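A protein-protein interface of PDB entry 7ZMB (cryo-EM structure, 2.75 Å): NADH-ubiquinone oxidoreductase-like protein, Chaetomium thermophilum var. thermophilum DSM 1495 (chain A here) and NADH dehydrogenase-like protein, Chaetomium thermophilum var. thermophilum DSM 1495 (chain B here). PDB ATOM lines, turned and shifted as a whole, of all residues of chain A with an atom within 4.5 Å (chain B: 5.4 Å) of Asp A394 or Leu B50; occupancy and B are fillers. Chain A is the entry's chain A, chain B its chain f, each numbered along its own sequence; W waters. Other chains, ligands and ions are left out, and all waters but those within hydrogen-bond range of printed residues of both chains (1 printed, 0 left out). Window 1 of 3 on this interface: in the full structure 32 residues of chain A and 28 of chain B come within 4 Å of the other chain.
The side-chain amide oxygen (OE1) of Gln A680 sits at hydrogen-bond distance from the backbone NH (N) of Val A393, at 3.4 Å. The backbone NH of Arg B51 sits at hydrogen-bond distance from the backbone carbonyl oxygen of Phe B16 (2.9 Å). The side-chain amide nitrogen (NE2) of Gln A680 is in hydrogen-bond range of the side-chain carboxylate (OD2) of Asp A394 (2.6 Å). The backbone NH of Phe B16 is in hydrogen-bond range of the backbone carbonyl oxygen of Leu B49, at 3.0 Å. The backbone carbonyl oxygen of Arg B51 is in hydrogen-bond range of the backbone NH of Phe B18. O of Ile B46 is in hydrogen-bond range of NZ of Lys B40 (3.0 Å).
Asp A394 touches just these residues of chain B: Tyr B36 (2.8 Å), Lys B40 (3.1 Å), Pro B47 (3.5 Å), Ile B48 (2.8 Å), Leu B49 (3.7 Å), Leu B50 (2.7 Å) and Arg B51 (2.9 Å). Printed residues of chain B within 4 Å of Gln A680: Tyr B36 and Lys B40. Phe B18 touches none of the printed residues of chain A. Of the printed residues of chain A, Leu B32 touches Leu A676 (3.8 Å). Printed residues of chain A within 4 Å of Tyr B36: Asp A394 (2.8 Å), Ile A395 (3.4 Å), Leu A676 (3.6 Å) and Gln A680 (3.6 Å). Of chain A, only Asp A394, Ile A395 and Leu A676 come within 4 Å of Leu B50. The nearest printed residue of chain A that does not touch Leu B50 is Arg A396 (4.5 Å).
N of Ile B48 lies within hydrogen-bond range of OD1 of Asp A394. The side-chain carboxylate (OD2) of Asp A394 lies within salt-bridge range of the side-chain amino group (NZ) of Lys B40 (3.1 Å). O of Asp A394 lies within hydrogen-bond range of N of Leu B50 (2.7 Å). The side-chain amide nitrogen (NE2) of Gln A680 lies close to the side-chain amino group (NZ) of Lys B40 (3.2 Å). The guanidinium group of Arg B51 is in hydrogen-bond range of the backbone carbonyl oxygen of Val A393, 2.4 Å away. The side-chain carboxylate (OD2) of Asp A394 lies within hydrogen-bond range of the side-chain hydroxyl (OH) of Tyr B36. O of Asp A394 sits at hydrogen-bond distance from NH2 of Arg B51, at 2.9 Å.
Of the 7 printed residues of chain A, 6 touch a printed residue of chain B. Printed residues of chain A that touch a printed residue of chain B: Val A393, Asp A394, Ile A395, Arg A396, Leu A676 and Gln A680. Among the printed residues, 17 pairs touch across the chains. Among the printed residues, Asp or Glu carboxylates within 4 Å of a Lys or Arg side-chain nitrogen of the other chain: Asp A394 with Lys B40 (3.1 Å).
Among the printed residues, merely in contact across the chains: Val A393 with Leu B49, Asp A394 with Pro B47, Asp A394 with Leu B49, Ile A395 with Tyr B36, Ile A395 with Leu B50, Arg A396 with Arg B51, Leu A676 with Leu B32, Leu A676 with Tyr B36, Leu A676 with Leu B50 and Gln A680 with Tyr B36.
Water W1 bridges O of Glu B52 (3.0 Å) and NE of Arg A396 (3.5 Å).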
ATOM      1  N   GLY A 392     -28.787   5.335 -26.125  1.00  0.00           N
ATOM      2  CA  GLY A 392     -27.505   4.715 -26.357  1.00  0.00           C
ATOM      3  C   GLY A 392     -27.648   3.213 -26.334  1.00  0.00           C
ATOM      4  O   GLY A 392     -28.733   2.660 -26.521  1.00  0.00           O
ATOM      5  N   VAL A 393     -26.531   2.540 -26.091  1.00  0.00           N
ATOM      6  CA  VAL A 393     -26.554   1.089 -26.020  1.00  0.00           C
ATOM      7  C   VAL A 393     -25.805   0.583 -24.792  1.00  0.00           C
ATOM      8  O   VAL A 393     -25.496  -0.609 -24.702  1.00  0.00           O
ATOM      9  CB  VAL A 393     -25.988   0.482 -27.315  1.00  0.00           C
ATOM     10  CG1 VAL A 393     -26.933   0.751 -28.474  1.00  0.00           C
ATOM     11  CG2 VAL A 393     -24.611   1.042 -27.617  1.00  0.00           C
ATOM     12  N   ASP A 394     -25.519   1.471 -23.830  1.00  0.00           N
ATOM     13  CA  ASP A 394     -24.742   1.061 -22.658  1.00  0.00           C
ATOM     14  C   ASP A 394     -25.547   0.156 -21.738  1.00  0.00           C
ATOM     15  O   ASP A 394     -25.058  -0.886 -21.290  1.00  0.00           O
ATOM     16  CB  ASP A 394     -24.249   2.278 -21.882  1.00  0.00           C
ATOM     17  CG  ASP A 394     -23.190   3.059 -22.623  1.00  0.00           C
ATOM     18  OD1 ASP A 394     -22.440   2.462 -23.415  1.00  0.00           O
ATOM     19  OD2 ASP A 394     -23.102   4.279 -22.401  1.00  0.00           O
ATOM     20  N   ILE A 395     -26.776   0.547 -21.431  1.00  0.00           N
ATOM     21  CA  ILE A 395     -27.692  -0.242 -20.622  1.00  0.00           C
ATOM     22  C   ILE A 395     -28.763  -0.783 -21.554  1.00  0.00           C
ATOM     23  O   ILE A 395     -29.331  -0.030 -22.353  1.00  0.00           O
ATOM     24  CB  ILE A 395     -28.299   0.596 -19.482  1.00  0.00           C
ATOM     25  CG1 ILE A 395     -27.209   1.067 -18.523  1.00  0.00           C
ATOM     26  CG2 ILE A 395     -29.336  -0.188 -18.724  1.00  0.00           C
ATOM     27  CD1 ILE A 395     -26.591   2.366 -18.896  1.00  0.00           C
ATOM     28  N   ARG A 396     -29.022  -2.091 -21.470  1.00  0.00           N
ATOM     29  CA  ARG A 396     -29.951  -2.719 -22.404  1.00  0.00           C
ATOM     30  C   ARG A 396     -31.359  -2.169 -22.260  1.00  0.00           C
ATOM     31  O   ARG A 396     -32.115  -2.142 -23.235  1.00  0.00           O
ATOM     32  CB  ARG A 396     -29.985  -4.230 -22.208  1.00  0.00           C
ATOM     33  CG  ARG A 396     -28.734  -4.965 -22.594  1.00  0.00           C
ATOM     34  CD  ARG A 396     -28.763  -6.318 -21.959  1.00  0.00           C
ATOM     35  NE  ARG A 396     -29.567  -7.236 -22.762  1.00  0.00           N
ATOM     36  CZ  ARG A 396     -30.420  -8.126 -22.268  1.00  0.00           C
ATOM     37  NH1 ARG A 396     -30.597  -8.230 -20.960  1.00  0.00           N
ATOM     38  NH2 ARG A 396     -31.102  -8.906 -23.085  1.00  0.00           N
ATOM     39  N   LEU A 676     -29.715   3.144 -14.408  1.00  0.00           N
ATOM     40  CA  LEU A 676     -28.604   3.759 -15.119  1.00  0.00           C
ATOM     41  C   LEU A 676     -29.042   4.232 -16.496  1.00  0.00           C
ATOM     42  O   LEU A 676     -28.271   4.873 -17.214  1.00  0.00           O
ATOM     43  CB  LEU A 676     -27.437   2.782 -15.242  1.00  0.00           C
ATOM     44  CG  LEU A 676     -26.483   2.723 -14.056  1.00  0.00           C
ATOM     45  CD1 LEU A 676     -25.333   1.809 -14.384  1.00  0.00           C
ATOM     46  CD2 LEU A 676     -25.993   4.107 -13.693  1.00  0.00           C
ATOM     47  N   GLN A 680     -27.733   8.095 -20.545  1.00  0.00           N
ATOM     48  CA  GLN A 680     -27.809   8.285 -21.986  1.00  0.00           C
ATOM     49  C   GLN A 680     -29.163   8.834 -22.412  1.00  0.00           C
ATOM     50  O   GLN A 680     -29.271   9.450 -23.476  1.00  0.00           O
ATOM     51  CB  GLN A 680     -27.503   6.974 -22.706  1.00  0.00           C
ATOM     52  CG  GLN A 680     -26.070   6.879 -23.203  1.00  0.00           C
ATOM     53  CD  GLN A 680     -25.661   5.473 -23.577  1.00  0.00           C
ATOM     54  OE1 GLN A 680     -26.361   4.506 -23.285  1.00  0.00           O
ATOM     55  NE2 GLN A 680     -24.517   5.352 -24.234  1.00  0.00           N
ATOM     56  N   PHE B  16     -18.435  -4.257 -19.563  1.00  0.00           N
ATOM     57  CA  PHE B  16     -18.535  -4.944 -18.284  1.00  0.00           C
ATOM     58  C   PHE B  16     -19.528  -6.095 -18.388  1.00  0.00           C
ATOM     59  O   PHE B  16     -20.668  -5.902 -18.818  1.00  0.00           O
ATOM     60  CB  PHE B  16     -18.981  -3.979 -17.185  1.00  0.00           C
ATOM     61  CG  PHE B  16     -17.958  -2.940 -16.829  1.00  0.00           C
ATOM     62  CD1 PHE B  16     -17.829  -1.792 -17.581  1.00  0.00           C
ATOM     63  CD2 PHE B  16     -17.134  -3.108 -15.735  1.00  0.00           C
ATOM     64  CE1 PHE B  16     -16.899  -0.835 -17.254  1.00  0.00           C
ATOM     65  CE2 PHE B  16     -16.201  -2.150 -15.404  1.00  0.00           C
ATOM     66  CZ  PHE B  16     -16.083  -1.013 -16.169  1.00  0.00           C
ATOM     67  N   PHE B  18     -21.306  -8.624 -15.943  1.00  0.00           N
ATOM     68  CA  PHE B  18     -21.589  -8.953 -14.521  1.00  0.00           C
ATOM     69  C   PHE B  18     -22.869  -9.780 -14.477  1.00  0.00           C
ATOM     70  O   PHE B  18     -23.306 -10.224 -15.535  1.00  0.00           O
ATOM     71  CB  PHE B  18     -21.722  -7.668 -13.696  1.00  0.00           C
ATOM     72  CG  PHE B  18     -22.739  -6.674 -14.197  1.00  0.00           C
ATOM     73  CD1 PHE B  18     -22.461  -5.845 -15.271  1.00  0.00           C
ATOM     74  CD2 PHE B  18     -23.973  -6.553 -13.580  1.00  0.00           C
ATOM     75  CE1 PHE B  18     -23.399  -4.936 -15.729  1.00  0.00           C
ATOM     76  CE2 PHE B  18     -24.910  -5.640 -14.034  1.00  0.00           C
ATOM     77  CZ  PHE B  18     -24.620  -4.833 -15.107  1.00  0.00           C
ATOM     78  N   LEU B  32     -20.307   0.014 -10.635  1.00  0.00           N
ATOM     79  CA  LEU B  32     -20.957   0.506 -11.881  1.00  0.00           C
ATOM     80  C   LEU B  32     -22.090   1.464 -11.523  1.00  0.00           C
ATOM     81  O   LEU B  32     -22.236   2.482 -12.216  1.00  0.00           O
ATOM     82  CB  LEU B  32     -21.431  -0.669 -12.740  1.00  0.00           C
ATOM     83  CG  LEU B  32     -20.311  -1.486 -13.376  1.00  0.00           C
ATOM     84  CD1 LEU B  32     -20.853  -2.761 -13.998  1.00  0.00           C
ATOM     85  CD2 LEU B  32     -19.551  -0.655 -14.394  1.00  0.00           C
ATOM     86  N   TYR B  36     -20.548   4.495 -13.577  1.00  0.00           N
ATOM     87  CA  TYR B  36     -21.033   4.691 -14.941  1.00  0.00           C
ATOM     88  C   TYR B  36     -21.547   6.101 -15.220  1.00  0.00           C
ATOM     89  O   TYR B  36     -21.272   6.612 -16.317  1.00  0.00           O
ATOM     90  CB  TYR B  36     -22.109   3.646 -15.288  1.00  0.00           C
ATOM     91  CG  TYR B  36     -22.785   3.967 -16.596  1.00  0.00           C
ATOM     92  CD1 TYR B  36     -22.156   3.705 -17.804  1.00  0.00           C
ATOM     93  CD2 TYR B  36     -24.023   4.579 -16.625  1.00  0.00           C
ATOM     94  CE1 TYR B  36     -22.751   4.022 -19.000  1.00  0.00           C
ATOM     95  CE2 TYR B  36     -24.621   4.902 -17.810  1.00  0.00           C
ATOM     96  CZ  TYR B  36     -23.985   4.619 -18.996  1.00  0.00           C
ATOM     97  OH  TYR B  36     -24.593   4.937 -20.183  1.00  0.00           O
ATOM     98  N   LYS B  40     -19.156   8.100 -17.686  1.00  0.00           N
ATOM     99  CA  LYS B  40     -19.719   8.403 -18.997  1.00  0.00           C
ATOM    100  C   LYS B  40     -19.814   9.896 -19.267  1.00  0.00           C
ATOM    101  O   LYS B  40     -19.734  10.313 -20.425  1.00  0.00           O
ATOM    102  CB  LYS B  40     -21.114   7.778 -19.132  1.00  0.00           C
ATOM    103  CG  LYS B  40     -21.845   8.093 -20.414  1.00  0.00           C
ATOM    104  CD  LYS B  40     -21.639   6.999 -21.437  1.00  0.00           C
ATOM    105  CE  LYS B  40     -22.136   7.405 -22.802  1.00  0.00           C
ATOM    106  NZ  LYS B  40     -21.582   6.519 -23.856  1.00  0.00           N
ATOM    107  N   ILE B  46     -17.553   7.392 -25.902  1.00  0.00           N
ATOM    108  CA  ILE B  46     -17.063   6.020 -25.783  1.00  0.00           C
ATOM    109  C   ILE B  46     -18.183   5.150 -25.234  1.00  0.00           C
ATOM    110  O   ILE B  46     -18.784   5.506 -24.216  1.00  0.00           O
ATOM    111  CB  ILE B  46     -15.820   5.930 -24.882  1.00  0.00           C
ATOM    112  CG1 ILE B  46     -14.899   7.131 -25.098  1.00  0.00           C
ATOM    113  CG2 ILE B  46     -15.077   4.638 -25.146  1.00  0.00           C
ATOM    114  CD1 ILE B  46     -14.456   7.332 -26.534  1.00  0.00           C
ATOM    115  N   PRO B  47     -18.481   4.009 -25.852  1.00  0.00           N
ATOM    116  CA  PRO B  47     -19.519   3.126 -25.313  1.00  0.00           C
ATOM    117  C   PRO B  47     -18.994   2.324 -24.132  1.00  0.00           C
ATOM    118  O   PRO B  47     -17.973   1.643 -24.227  1.00  0.00           O
ATOM    119  CB  PRO B  47     -19.861   2.215 -26.494  1.00  0.00           C
ATOM    120  CG  PRO B  47     -18.692   2.261 -27.377  1.00  0.00           C
ATOM    121  CD  PRO B  47     -17.908   3.500 -27.109  1.00  0.00           C
ATOM    122  N   ILE B  48     -19.705   2.418 -23.013  1.00  0.00           N
ATOM    123  CA  ILE B  48     -19.452   1.573 -21.858  1.00  0.00           C
ATOM    124  C   ILE B  48     -20.592   0.569 -21.796  1.00  0.00           C
ATOM    125  O   ILE B  48     -21.594   0.796 -21.116  1.00  0.00           O
ATOM    126  CB  ILE B  48     -19.362   2.401 -20.563  1.00  0.00           C
ATOM    127  CG1 ILE B  48     -18.277   3.471 -20.676  1.00  0.00           C
ATOM    128  CG2 ILE B  48     -19.098   1.517 -19.359  1.00  0.00           C
ATOM    129  CD1 ILE B  48     -18.786   4.833 -21.038  1.00  0.00           C
ATOM    130  N   LEU B  49     -20.450  -0.551 -22.494  1.00  0.00           N
ATOM    131  CA  LEU B  49     -21.547  -1.501 -22.614  1.00  0.00           C
ATOM    132  C   LEU B  49     -21.666  -2.288 -21.316  1.00  0.00           C
ATOM    133  O   LEU B  49     -20.774  -3.065 -20.964  1.00  0.00           O
ATOM    134  CB  LEU B  49     -21.330  -2.429 -23.803  1.00  0.00           C
ATOM    135  CG  LEU B  49     -21.152  -1.838 -25.204  1.00  0.00           C
ATOM    136  CD1 LEU B  49     -21.514  -2.876 -26.243  1.00  0.00           C
ATOM    137  CD2 LEU B  49     -21.958  -0.556 -25.429  1.00  0.00           C
ATOM    138  N   LEU B  50     -22.763  -2.080 -20.600  1.00  0.00           N
ATOM    139  CA  LEU B  50     -23.075  -2.847 -19.402  1.00  0.00           C
ATOM    140  C   LEU B  50     -23.930  -4.039 -19.801  1.00  0.00           C
ATOM    141  O   LEU B  50     -25.103  -3.881 -20.152  1.00  0.00           O
ATOM    142  CB  LEU B  50     -23.790  -1.972 -18.380  1.00  0.00           C
ATOM    143  CG  LEU B  50     -22.988  -0.732 -17.996  1.00  0.00           C
ATOM    144  CD1 LEU B  50     -23.839   0.267 -17.258  1.00  0.00           C
ATOM    145  CD2 LEU B  50     -21.812  -1.151 -17.163  1.00  0.00           C
ATOM    146  N   ARG B  51     -23.346  -5.228 -19.755  1.00  0.00           N
ATOM    147  CA  ARG B  51     -24.018  -6.449 -20.178  1.00  0.00           C
ATOM    148  C   ARG B  51     -24.013  -7.443 -19.033  1.00  0.00           C
ATOM    149  O   ARG B  51     -22.969  -7.691 -18.428  1.00  0.00           O
ATOM    150  CB  ARG B  51     -23.339  -7.046 -21.410  1.00  0.00           C
ATOM    151  CG  ARG B  51     -23.278  -6.077 -22.560  1.00  0.00           C
ATOM    152  CD  ARG B  51     -24.666  -5.820 -23.081  1.00  0.00           C
ATOM    153  NE  ARG B  51     -24.675  -4.932 -24.234  1.00  0.00           N
ATOM    154  CZ  ARG B  51     -25.055  -3.663 -24.179  1.00  0.00           C
ATOM    155  NH1 ARG B  51     -25.040  -2.919 -25.274  1.00  0.00           N
ATOM    156  NH2 ARG B  51     -25.449  -3.143 -23.027  1.00  0.00           N
ATOM    157  N   GLU B  52     -25.169  -8.008 -18.733  1.00  0.00           N
ATOM    158  CA  GLU B  52     -25.291  -8.909 -17.606  1.00  0.00           C
ATOM    159  C   GLU B  52     -26.083 -10.144 -18.002  1.00  0.00           C
ATOM    160  O   GLU B  52     -26.909 -10.113 -18.915  1.00  0.00           O
ATOM    161  CB  GLU B  52     -25.935  -8.215 -16.395  1.00  0.00           C
ATOM    162  CG  GLU B  52     -27.351  -7.760 -16.598  1.00  0.00           C
ATOM    163  CD  GLU B  52     -27.441  -6.326 -17.061  1.00  0.00           C
ATOM    164  OE1 GLU B  52     -26.519  -5.854 -17.756  1.00  0.00           O
ATOM    165  OE2 GLU B  52     -28.429  -5.655 -16.712  1.00  0.00           O
HETATM  166  O   HOH W   1     -26.674  -8.723 -21.563  1.00  0.00           O
